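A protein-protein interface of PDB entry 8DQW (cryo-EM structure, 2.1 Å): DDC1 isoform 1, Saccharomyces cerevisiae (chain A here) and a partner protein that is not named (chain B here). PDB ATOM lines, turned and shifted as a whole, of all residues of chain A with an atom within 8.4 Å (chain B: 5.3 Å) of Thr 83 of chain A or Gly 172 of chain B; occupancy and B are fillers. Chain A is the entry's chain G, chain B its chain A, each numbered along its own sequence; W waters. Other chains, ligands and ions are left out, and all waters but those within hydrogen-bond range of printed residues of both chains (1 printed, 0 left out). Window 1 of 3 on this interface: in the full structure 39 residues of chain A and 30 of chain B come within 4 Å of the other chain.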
ATOM      1  N   ILE A  60      24.840   3.372  28.847  1.00  0.00           N
ATOM      2  CA  ILE A  60      23.906   3.749  27.787  1.00  0.00           C
ATOM      3  C   ILE A  60      23.817   5.268  27.651  1.00  0.00           C
ATOM      4  O   ILE A  60      23.887   5.810  26.542  1.00  0.00           O
ATOM      5  CB  ILE A  60      22.526   3.119  28.039  1.00  0.00           C
ATOM      6  CG1 ILE A  60      22.579   1.626  27.718  1.00  0.00           C
ATOM      7  CG2 ILE A  60      21.461   3.810  27.190  1.00  0.00           C
ATOM      8  CD1 ILE A  60      21.433   0.842  28.283  1.00  0.00           C
ATOM      9  N   SER A  77      17.210   4.255  31.016  1.00  0.00           N
ATOM     10  CA  SER A  77      18.139   5.073  30.256  1.00  0.00           C
ATOM     11  C   SER A  77      17.848   4.914  28.769  1.00  0.00           C
ATOM     12  O   SER A  77      17.454   3.838  28.307  1.00  0.00           O
ATOM     13  CB  SER A  77      19.590   4.688  30.565  1.00  0.00           C
ATOM     14  OG  SER A  77      20.500   5.483  29.833  1.00  0.00           O
ATOM     15  N   MET A  78      18.036   6.008  28.031  1.00  0.00           N
ATOM     16  CA  MET A  78      17.881   6.031  26.583  1.00  0.00           C
ATOM     17  C   MET A  78      19.024   6.837  25.986  1.00  0.00           C
ATOM     18  O   MET A  78      19.381   7.897  26.507  1.00  0.00           O
ATOM     19  CB  MET A  78      16.531   6.638  26.172  1.00  0.00           C
ATOM     20  CG  MET A  78      16.203   6.489  24.691  1.00  0.00           C
ATOM     21  SD  MET A  78      14.441   6.628  24.320  1.00  0.00           S
ATOM     22  CE  MET A  78      13.930   7.872  25.504  1.00  0.00           C
ATOM     23  N   ASN A  79      19.596   6.335  24.894  1.00  0.00           N
ATOM     24  CA  ASN A  79      20.751   6.983  24.294  1.00  0.00           C
ATOM     25  C   ASN A  79      20.324   8.220  23.501  1.00  0.00           C
ATOM     26  O   ASN A  79      19.138   8.477  23.280  1.00  0.00           O
ATOM     27  CB  ASN A  79      21.515   6.003  23.403  1.00  0.00           C
ATOM     28  CG  ASN A  79      20.805   5.720  22.093  1.00  0.00           C
ATOM     29  OD1 ASN A  79      19.591   5.885  21.977  1.00  0.00           O
ATOM     30  ND2 ASN A  79      21.564   5.274  21.099  1.00  0.00           N
ATOM     31  N   GLU A  80      21.324   8.994  23.072  1.00  0.00           N
ATOM     32  CA  GLU A  80      21.051  10.273  22.422  1.00  0.00           C
ATOM     33  C   GLU A  80      20.238  10.088  21.145  1.00  0.00           C
ATOM     34  O   GLU A  80      19.302  10.852  20.882  1.00  0.00           O
ATOM     35  CB  GLU A  80      22.362  10.995  22.118  1.00  0.00           C
ATOM     36  CG  GLU A  80      23.188  11.339  23.349  1.00  0.00           C
ATOM     37  CD  GLU A  80      22.526  12.389  24.224  1.00  0.00           C
ATOM     38  OE1 GLU A  80      22.679  12.315  25.460  1.00  0.00           O
ATOM     39  OE2 GLU A  80      21.852  13.285  23.674  1.00  0.00           O
ATOM     40  N   THR A  81      20.575   9.080  20.342  1.00  0.00           N
ATOM     41  CA  THR A  81      19.899   8.849  19.071  1.00  0.00           C
ATOM     42  C   THR A  81      18.536   8.188  19.231  1.00  0.00           C
ATOM     43  O   THR A  81      17.848   7.983  18.226  1.00  0.00           O
ATOM     44  CB  THR A  81      20.775   7.987  18.157  1.00  0.00           C
ATOM     45  OG1 THR A  81      21.164   6.792  18.845  1.00  0.00           O
ATOM     46  CG2 THR A  81      22.017   8.754  17.727  1.00  0.00           C
ATOM     47  N   ASP A  82      18.136   7.841  20.454  1.00  0.00           N
ATOM     48  CA  ASP A  82      16.851   7.191  20.709  1.00  0.00           C
ATOM     49  C   ASP A  82      16.752   5.843  20.000  1.00  0.00           C
ATOM     50  O   ASP A  82      15.661   5.397  19.636  1.00  0.00           O
ATOM     51  CB  ASP A  82      15.682   8.094  20.299  1.00  0.00           C
ATOM     52  CG  ASP A  82      15.394   9.174  21.320  1.00  0.00           C
ATOM     53  OD1 ASP A  82      16.327   9.923  21.678  1.00  0.00           O
ATOM     54  OD2 ASP A  82      14.230   9.275  21.765  1.00  0.00           O
ATOM     55  N   THR A  83      17.891   5.182  19.795  1.00  0.00           N
ATOM     56  CA  THR A  83      17.923   3.871  19.162  1.00  0.00           C
ATOM     57  C   THR A  83      17.977   2.722  20.161  1.00  0.00           C
ATOM     58  O   THR A  83      17.874   1.562  19.749  1.00  0.00           O
ATOM     59  CB  THR A  83      19.124   3.768  18.213  1.00  0.00           C
ATOM     60  OG1 THR A  83      20.306   4.232  18.878  1.00  0.00           O
ATOM     61  CG2 THR A  83      18.889   4.600  16.959  1.00  0.00           C
ATOM     62  N   THR A  84      18.132   3.009  21.453  1.00  0.00           N
ATOM     63  CA  THR A  84      18.194   1.965  22.465  1.00  0.00           C
ATOM     64  C   THR A  84      17.576   2.476  23.758  1.00  0.00           C
ATOM     65  O   THR A  84      17.817   3.616  24.163  1.00  0.00           O
ATOM     66  CB  THR A  84      19.637   1.515  22.725  1.00  0.00           C
ATOM     67  OG1 THR A  84      19.659   0.577  23.809  1.00  0.00           O
ATOM     68  CG2 THR A  84      20.513   2.706  23.080  1.00  0.00           C
ATOM     69  N   LEU A  85      16.782   1.621  24.396  1.00  0.00           N
ATOM     70  CA  LEU A  85      16.165   1.912  25.684  1.00  0.00           C
ATOM     71  C   LEU A  85      16.408   0.730  26.609  1.00  0.00           C
ATOM     72  O   LEU A  85      16.160  -0.417  26.226  1.00  0.00           O
ATOM     73  CB  LEU A  85      14.660   2.174  25.525  1.00  0.00           C
ATOM     74  CG  LEU A  85      13.818   2.493  26.769  1.00  0.00           C
ATOM     75  CD1 LEU A  85      13.343   1.222  27.468  1.00  0.00           C
ATOM     76  CD2 LEU A  85      14.575   3.387  27.741  1.00  0.00           C
ATOM     77  N   CYS A  86      16.901   1.001  27.815  1.00  0.00           N
ATOM     78  CA  CYS A  86      17.106  -0.029  28.823  1.00  0.00           C
ATOM     79  C   CYS A  86      16.348   0.345  30.086  1.00  0.00           C
ATOM     80  O   CYS A  86      16.335   1.514  30.491  1.00  0.00           O
ATOM     81  CB  CYS A  86      18.591  -0.218  29.136  1.00  0.00           C
ATOM     82  SG  CYS A  86      18.944  -1.569  30.288  1.00  0.00           S
ATOM     83  N   ASP A 284      30.722  -4.230  15.169  1.00  0.00           N
ATOM     84  CA  ASP A 284      29.731  -3.309  15.706  1.00  0.00           C
ATOM     85  C   ASP A 284      28.293  -3.700  15.388  1.00  0.00           C
ATOM     86  O   ASP A 284      27.373  -3.085  15.938  1.00  0.00           O
ATOM     87  CB  ASP A 284      30.001  -1.890  15.185  1.00  0.00           C
ATOM     88  CG  ASP A 284      29.419  -1.649  13.806  1.00  0.00           C
ATOM     89  OD1 ASP A 284      28.188  -1.468  13.702  1.00  0.00           O
ATOM     90  OD2 ASP A 284      30.191  -1.640  12.825  1.00  0.00           O
ATOM     91  N   PHE A 358      20.958  -5.462  14.208  1.00  0.00           N
ATOM     92  CA  PHE A 358      20.929  -4.326  15.123  1.00  0.00           C
ATOM     93  C   PHE A 358      22.325  -4.124  15.702  1.00  0.00           C
ATOM     94  O   PHE A 358      23.288  -4.785  15.304  1.00  0.00           O
ATOM     95  CB  PHE A 358      19.872  -4.520  16.218  1.00  0.00           C
ATOM     96  CG  PHE A 358      19.918  -5.865  16.887  1.00  0.00           C
ATOM     97  CD1 PHE A 358      19.273  -6.956  16.328  1.00  0.00           C
ATOM     98  CD2 PHE A 358      20.591  -6.035  18.086  1.00  0.00           C
ATOM     99  CE1 PHE A 358      19.309  -8.192  16.945  1.00  0.00           C
ATOM    100  CE2 PHE A 358      20.629  -7.270  18.709  1.00  0.00           C
ATOM    101  CZ  PHE A 358      19.988  -8.349  18.137  1.00  0.00           C
ATOM    102  N   LYS A 359      22.433  -3.170  16.623  1.00  0.00           N
ATOM    103  CA  LYS A 359      23.706  -2.863  17.257  1.00  0.00           C
ATOM    104  C   LYS A 359      24.017  -3.880  18.349  1.00  0.00           C
ATOM    105  O   LYS A 359      23.120  -4.392  19.025  1.00  0.00           O
ATOM    106  CB  LYS A 359      23.689  -1.452  17.845  1.00  0.00           C
ATOM    107  CG  LYS A 359      24.882  -0.605  17.441  1.00  0.00           C
ATOM    108  CD  LYS A 359      24.812   0.788  18.042  1.00  0.00           C
ATOM    109  CE  LYS A 359      26.154   1.490  17.958  1.00  0.00           C
ATOM    110  NZ  LYS A 359      27.099   1.017  19.005  1.00  0.00           N
ATOM    111  N   ASP A 362      25.136  -2.557  23.071  1.00  0.00           N
ATOM    112  CA  ASP A 362      24.128  -2.511  24.125  1.00  0.00           C
ATOM    113  C   ASP A 362      23.654  -3.908  24.496  1.00  0.00           C
ATOM    114  O   ASP A 362      23.458  -4.207  25.677  1.00  0.00           O
ATOM    115  CB  ASP A 362      22.949  -1.646  23.686  1.00  0.00           C
ATOM    116  CG  ASP A 362      23.190  -0.173  23.930  1.00  0.00           C
ATOM    117  OD1 ASP A 362      24.349   0.210  24.193  1.00  0.00           O
ATOM    118  OD2 ASP A 362      22.218   0.603  23.859  1.00  0.00           O
ATOM    119  N   PRO A 393      11.190  -2.220  16.150  1.00  0.00           N
ATOM    120  CA  PRO A 393      12.015  -2.471  17.336  1.00  0.00           C
ATOM    121  C   PRO A 393      12.086  -3.950  17.683  1.00  0.00           C
ATOM    122  O   PRO A 393      11.149  -4.717  17.449  1.00  0.00           O
ATOM    123  CB  PRO A 393      11.310  -1.678  18.445  1.00  0.00           C
ATOM    124  CG  PRO A 393      10.343  -0.778  17.753  1.00  0.00           C
ATOM    125  CD  PRO A 393       9.975  -1.457  16.480  1.00  0.00           C
ATOM    126  N   ILE A 394      13.223  -4.341  18.252  1.00  0.00           N
ATOM    127  CA  ILE A 394      13.420  -5.667  18.826  1.00  0.00           C
ATOM    128  C   ILE A 394      13.416  -5.522  20.341  1.00  0.00           C
ATOM    129  O   ILE A 394      14.118  -4.663  20.893  1.00  0.00           O
ATOM    130  CB  ILE A 394      14.723  -6.324  18.337  1.00  0.00           C
ATOM    131  CG1 ILE A 394      14.883  -7.707  18.976  1.00  0.00           C
ATOM    132  CG2 ILE A 394      15.933  -5.457  18.662  1.00  0.00           C
ATOM    133  CD1 ILE A 394      15.943  -8.569  18.321  1.00  0.00           C
ATOM    134  N   LEU A 407      15.208  -4.485  27.314  1.00  0.00           N
ATOM    135  CA  LEU A 407      16.060  -3.784  26.359  1.00  0.00           C
ATOM    136  C   LEU A 407      15.331  -3.707  25.026  1.00  0.00           C
ATOM    137  O   LEU A 407      14.949  -4.736  24.466  1.00  0.00           O
ATOM    138  CB  LEU A 407      17.408  -4.494  26.195  1.00  0.00           C
ATOM    139  CG  LEU A 407      18.408  -3.836  25.241  1.00  0.00           C
ATOM    140  CD1 LEU A 407      19.132  -2.686  25.924  1.00  0.00           C
ATOM    141  CD2 LEU A 407      19.400  -4.860  24.714  1.00  0.00           C
ATOM    142  N   VAL A 408      15.150  -2.495  24.513  1.00  0.00           N
ATOM    143  CA  VAL A 408      14.499  -2.260  23.229  1.00  0.00           C
ATOM    144  C   VAL A 408      15.514  -1.607  22.305  1.00  0.00           C
ATOM    145  O   VAL A 408      16.180  -0.641  22.695  1.00  0.00           O
ATOM    146  CB  VAL A 408      13.246  -1.377  23.378  1.00  0.00           C
ATOM    147  CG1 VAL A 408      12.569  -1.185  22.028  1.00  0.00           C
ATOM    148  CG2 VAL A 408      12.282  -1.987  24.384  1.00  0.00           C
ATOM    149  N   GLU A 409      15.641  -2.136  21.089  1.00  0.00           N
ATOM    150  CA  GLU A 409      16.596  -1.612  20.121  1.00  0.00           C
ATOM    151  C   GLU A 409      15.911  -1.395  18.777  1.00  0.00           C
ATOM    152  O   GLU A 409      14.888  -2.009  18.472  1.00  0.00           O
ATOM    153  CB  GLU A 409      17.800  -2.549  19.953  1.00  0.00           C
ATOM    154  CG  GLU A 409      19.012  -2.151  20.786  1.00  0.00           C
ATOM    155  CD  GLU A 409      20.278  -2.881  20.375  1.00  0.00           C
ATOM    156  OE1 GLU A 409      20.417  -3.211  19.179  1.00  0.00           O
ATOM    157  OE2 GLU A 409      21.137  -3.122  21.248  1.00  0.00           O
ATOM    158  N   VAL A 410      16.488  -0.503  17.978  1.00  0.00           N
ATOM    159  CA  VAL A 410      16.002  -0.236  16.629  1.00  0.00           C
ATOM    160  C   VAL A 410      16.740  -1.149  15.658  1.00  0.00           C
ATOM    161  O   VAL A 410      17.972  -1.251  15.701  1.00  0.00           O
ATOM    162  CB  VAL A 410      16.197   1.243  16.253  1.00  0.00           C
ATOM    163  CG1 VAL A 410      15.929   1.458  14.769  1.00  0.00           C
ATOM    164  CG2 VAL A 410      15.293   2.130  17.096  1.00  0.00           C
ATOM    165  N   THR A 411      15.990  -1.814  14.786  1.00  0.00           N
ATOM    166  CA  THR A 411      16.541  -2.777  13.844  1.00  0.00           C
ATOM    167  C   THR A 411      16.742  -2.142  12.470  1.00  0.00           C
ATOM    168  O   THR A 411      16.126  -1.131  12.127  1.00  0.00           O
ATOM    169  CB  THR A 411      15.624  -3.999  13.721  1.00  0.00           C
ATOM    170  OG1 THR A 411      14.331  -3.587  13.263  1.00  0.00           O
ATOM    171  CG2 THR A 411      15.485  -4.704  15.064  1.00  0.00           C
ATOM    172  N   PHE B 139       8.069   3.750  20.083  1.00  0.00           N
ATOM    173  CA  PHE B 139       8.551   3.665  21.457  1.00  0.00           C
ATOM    174  C   PHE B 139       7.417   3.912  22.445  1.00  0.00           C
ATOM    175  O   PHE B 139       7.025   3.017  23.202  1.00  0.00           O
ATOM    176  CB  PHE B 139       9.688   4.666  21.675  1.00  0.00           C
ATOM    177  CG  PHE B 139      11.052   4.120  21.351  1.00  0.00           C
ATOM    178  CD1 PHE B 139      11.256   3.347  20.219  1.00  0.00           C
ATOM    179  CD2 PHE B 139      12.131   4.382  22.179  1.00  0.00           C
ATOM    180  CE1 PHE B 139      12.510   2.845  19.920  1.00  0.00           C
ATOM    181  CE2 PHE B 139      13.388   3.882  21.885  1.00  0.00           C
ATOM    182  CZ  PHE B 139      13.577   3.113  20.755  1.00  0.00           C
ATOM    183  N   GLU B 168      30.442   6.456  17.934  1.00  0.00           N
ATOM    184  CA  GLU B 168      29.243   5.770  18.400  1.00  0.00           C
ATOM    185  C   GLU B 168      27.989   6.457  17.873  1.00  0.00           C
ATOM    186  O   GLU B 168      27.077   5.800  17.355  1.00  0.00           O
ATOM    187  CB  GLU B 168      29.234   5.715  19.927  1.00  0.00           C
ATOM    188  CG  GLU B 168      28.426   4.563  20.507  1.00  0.00           C
ATOM    189  CD  GLU B 168      29.049   3.207  20.227  1.00  0.00           C
ATOM    190  OE1 GLU B 168      30.219   3.161  19.793  1.00  0.00           O
ATOM    191  OE2 GLU B 168      28.366   2.184  20.444  1.00  0.00           O
ATOM    192  N   PHE B 169      27.949   7.789  17.955  1.00  0.00           N
ATOM    193  CA  PHE B 169      26.748   8.520  17.562  1.00  0.00           C
ATOM    194  C   PHE B 169      26.332   8.164  16.141  1.00  0.00           C
ATOM    195  O   PHE B 169      25.190   7.754  15.896  1.00  0.00           O
ATOM    196  CB  PHE B 169      26.994  10.025  17.692  1.00  0.00           C
ATOM    197  CG  PHE B 169      25.871  10.872  17.166  1.00  0.00           C
ATOM    198  CD1 PHE B 169      24.684  10.986  17.869  1.00  0.00           C
ATOM    199  CD2 PHE B 169      26.005  11.559  15.971  1.00  0.00           C
ATOM    200  CE1 PHE B 169      23.649  11.766  17.388  1.00  0.00           C
ATOM    201  CE2 PHE B 169      24.972  12.341  15.484  1.00  0.00           C
ATOM    202  CZ  PHE B 169      23.794  12.445  16.196  1.00  0.00           C
ATOM    203  N   LEU B 170      27.264   8.276  15.193  1.00  0.00           N
ATOM    204  CA  LEU B 170      26.938   7.957  13.808  1.00  0.00           C
ATOM    205  C   LEU B 170      26.477   6.513  13.678  1.00  0.00           C
ATOM    206  O   LEU B 170      25.531   6.219  12.937  1.00  0.00           O
ATOM    207  CB  LEU B 170      28.145   8.223  12.907  1.00  0.00           C
ATOM    208  CG  LEU B 170      28.556   9.688  12.729  1.00  0.00           C
ATOM    209  CD1 LEU B 170      29.722   9.800  11.755  1.00  0.00           C
ATOM    210  CD2 LEU B 170      27.387  10.547  12.260  1.00  0.00           C
ATOM    211  N   LYS B 171      27.112   5.596  14.414  1.00  0.00           N
ATOM    212  CA  LYS B 171      26.725   4.195  14.319  1.00  0.00           C
ATOM    213  C   LYS B 171      25.276   3.979  14.732  1.00  0.00           C
ATOM    214  O   LYS B 171      24.663   2.994  14.309  1.00  0.00           O
ATOM    215  CB  LYS B 171      27.655   3.332  15.171  1.00  0.00           C
ATOM    216  CG  LYS B 171      29.000   3.074  14.514  1.00  0.00           C
ATOM    217  CD  LYS B 171      29.947   2.325  15.436  1.00  0.00           C
ATOM    218  CE  LYS B 171      31.177   1.846  14.683  1.00  0.00           C
ATOM    219  NZ  LYS B 171      31.890   2.963  14.000  1.00  0.00           N
ATOM    220  N   GLY B 172      24.715   4.876  15.537  1.00  0.00           N
ATOM    221  CA  GLY B 172      23.297   4.824  15.829  1.00  0.00           C
ATOM    222  C   GLY B 172      22.506   5.613  14.807  1.00  0.00           C
ATOM    223  O   GLY B 172      21.432   5.190  14.367  1.00  0.00           O
ATOM    224  N   ALA B 173      23.057   6.760  14.400  1.00  0.00           N
ATOM    225  CA  ALA B 173      22.337   7.651  13.496  1.00  0.00           C
ATOM    226  C   ALA B 173      21.992   6.963  12.184  1.00  0.00           C
ATOM    227  O   ALA B 173      21.002   7.324  11.538  1.00  0.00           O
ATOM    228  CB  ALA B 173      23.165   8.908  13.234  1.00  0.00           C
ATOM    229  N   ARG B 174      22.786   5.971  11.774  1.00  0.00           N
ATOM    230  CA  ARG B 174      22.518   5.290  10.512  1.00  0.00           C
ATOM    231  C   ARG B 174      21.164   4.595  10.526  1.00  0.00           C
ATOM    232  O   ARG B 174      20.557   4.402   9.467  1.00  0.00           O
ATOM    233  CB  ARG B 174      23.641   4.289  10.208  1.00  0.00           C
ATOM    234  CG  ARG B 174      23.275   2.809  10.360  1.00  0.00           C
ATOM    235  CD  ARG B 174      24.349   1.913   9.767  1.00  0.00           C
ATOM    236  NE  ARG B 174      24.167   0.515  10.134  1.00  0.00           N
ATOM    237  CZ  ARG B 174      23.175  -0.255   9.702  1.00  0.00           C
ATOM    238  NH1 ARG B 174      22.248   0.206   8.880  1.00  0.00           N
ATOM    239  NH2 ARG B 174      23.114  -1.521  10.106  1.00  0.00           N
ATOM    240  N   TYR B 175      20.672   4.209  11.705  1.00  0.00           N
ATOM    241  CA  TYR B 175      19.432   3.445  11.784  1.00  0.00           C
ATOM    242  C   TYR B 175      18.182   4.303  11.635  1.00  0.00           C
ATOM    243  O   TYR B 175      17.089   3.747  11.480  1.00  0.00           O
ATOM    244  CB  TYR B 175      19.367   2.688  13.115  1.00  0.00           C
ATOM    245  CG  TYR B 175      20.237   1.453  13.167  1.00  0.00           C
ATOM    246  CD1 TYR B 175      21.565   1.532  13.565  1.00  0.00           C
ATOM    247  CD2 TYR B 175      19.730   0.206  12.823  1.00  0.00           C
ATOM    248  CE1 TYR B 175      22.366   0.407  13.615  1.00  0.00           C
ATOM    249  CE2 TYR B 175      20.523  -0.926  12.871  1.00  0.00           C
ATOM    250  CZ  TYR B 175      21.838  -0.820  13.268  1.00  0.00           C
ATOM    251  OH  TYR B 175      22.631  -1.943  13.317  1.00  0.00           O
ATOM    252  N   LEU B 176      18.307   5.628  11.673  1.00  0.00           N
ATOM    253  CA  LEU B 176      17.146   6.519  11.672  1.00  0.00           C
ATOM    254  C   LEU B 176      16.711   6.808  10.234  1.00  0.00           C
ATOM    255  O   LEU B 176      16.869   7.907   9.701  1.00  0.00           O
ATOM    256  CB  LEU B 176      17.466   7.801  12.431  1.00  0.00           C
ATOM    257  CG  LEU B 176      17.992   7.597  13.854  1.00  0.00           C
ATOM    258  CD1 LEU B 176      18.487   8.908  14.440  1.00  0.00           C
ATOM    259  CD2 LEU B 176      16.916   6.980  14.735  1.00  0.00           C
HETATM  260  O   HOH W   1      15.876   1.311  10.619  1.00  0.00           O
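The side-chain amino group (NZ) of Lys 359 of chain A lies within salt-bridge range of the side-chain carboxylate (OE1) of Glu 168 of chain B (3.9 Å).
Hydrophobic or aromatic side chains of chain A that line the printed part of chain B: Met 78.
Printed residues of chain B that touch a printed residue of chain A: Phe 139, Glu 168, Phe 169, Lys 171, Gly 172, Tyr 175 and Leu 176.
Among the printed residues, Asp or Glu carboxylates within 4 Å of a Lys or Arg side-chain nitrogen of the other chain: Lys 359 of chain A with Glu 168 of chain B.
Of chain B, only Gly 172 and Leu 176 come within 4 Å of Thr 83 of chain A.
Gly 172 of chain B touches one residue of chain A.
Of the printed residues of chain B, Thr 411 of chain A touches Tyr 175.
Of the printed residues of chain A, Lys 171 of chain B touches Asp 284 and Lys 359.
Glu 80 of chain A touches none of the printed residues of chain B.
Pro 393 of chain A touches none of the printed residues of chain B.
The nearest printed residue of chain A that does not touch Phe 139 of chain B is Val 410 of chain A (4.03 Å).
Water W1 lies within hydrogen-bond range of the backbone carbonyl oxygen of Tyr 175 of chain B (2.9 Å) and the backbone carbonyl oxygen of Thr 411 of chain A (2.9 Å).
The side-chain amide oxygen of Asn 79 of chain A sits at hydrogen-bond distance from the backbone NH of Asp 82 of chain A, at 2.9 Å.
OH of Tyr 175 of chain B is in hydrogen-bond range of NH2 of Arg 174 of chain B.
The backbone NH (N) of Lys 359 of chain A sits at hydrogen-bond distance from the side-chain carboxylate (OE1) of Glu 409 of chain A.
The side-chain hydroxyl (OG1) of Thr 81 of chain A is in hydrogen-bond range of the side-chain amide nitrogen (ND2) of Asn 79 of chain A (2.7 Å).
The backbone carbonyl oxygen (O) of Thr 83 of chain A is in hydrogen-bond range of the backbone NH (N) of Val 410 of chain A (3.1 Å).
The side-chain hydroxyl of Thr 83 of chain A lies within hydrogen-bond range of the side-chain hydroxyl of Thr 81 of chain A, at 2.7 Å.
Among the printed residues, merely in contact across the chains: Met 78 of chain A with Phe 139 of chain B (3.8 Å), Thr 81 of chain A with Phe 169 of chain B (3.4 Å), Thr 81 of chain A with Leu 176 of chain B (3.7 Å), Asp 82 of chain A with Phe 139 of chain B (3.3 Å), Thr 83 of chain A with Gly 172 of chain B (3.7 Å), Thr 83 of chain A with Leu 176 of chain B (3.8 Å), Asp 284 of chain A with Lys 171 of chain B (3.9 Å), Phe 358 of chain A with Tyr 175 of chain B (3.2 Å), Lys 359 of chain A with Lys 171 of chain B (3.7 Å), Lys 359 of chain A with Tyr 175 of chain B (3.5 Å), Val 410 of chain A with Tyr 175 of chain B (3.7 Å) and Thr 411 of chain A with Tyr 175 of chain B (3.8 Å).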
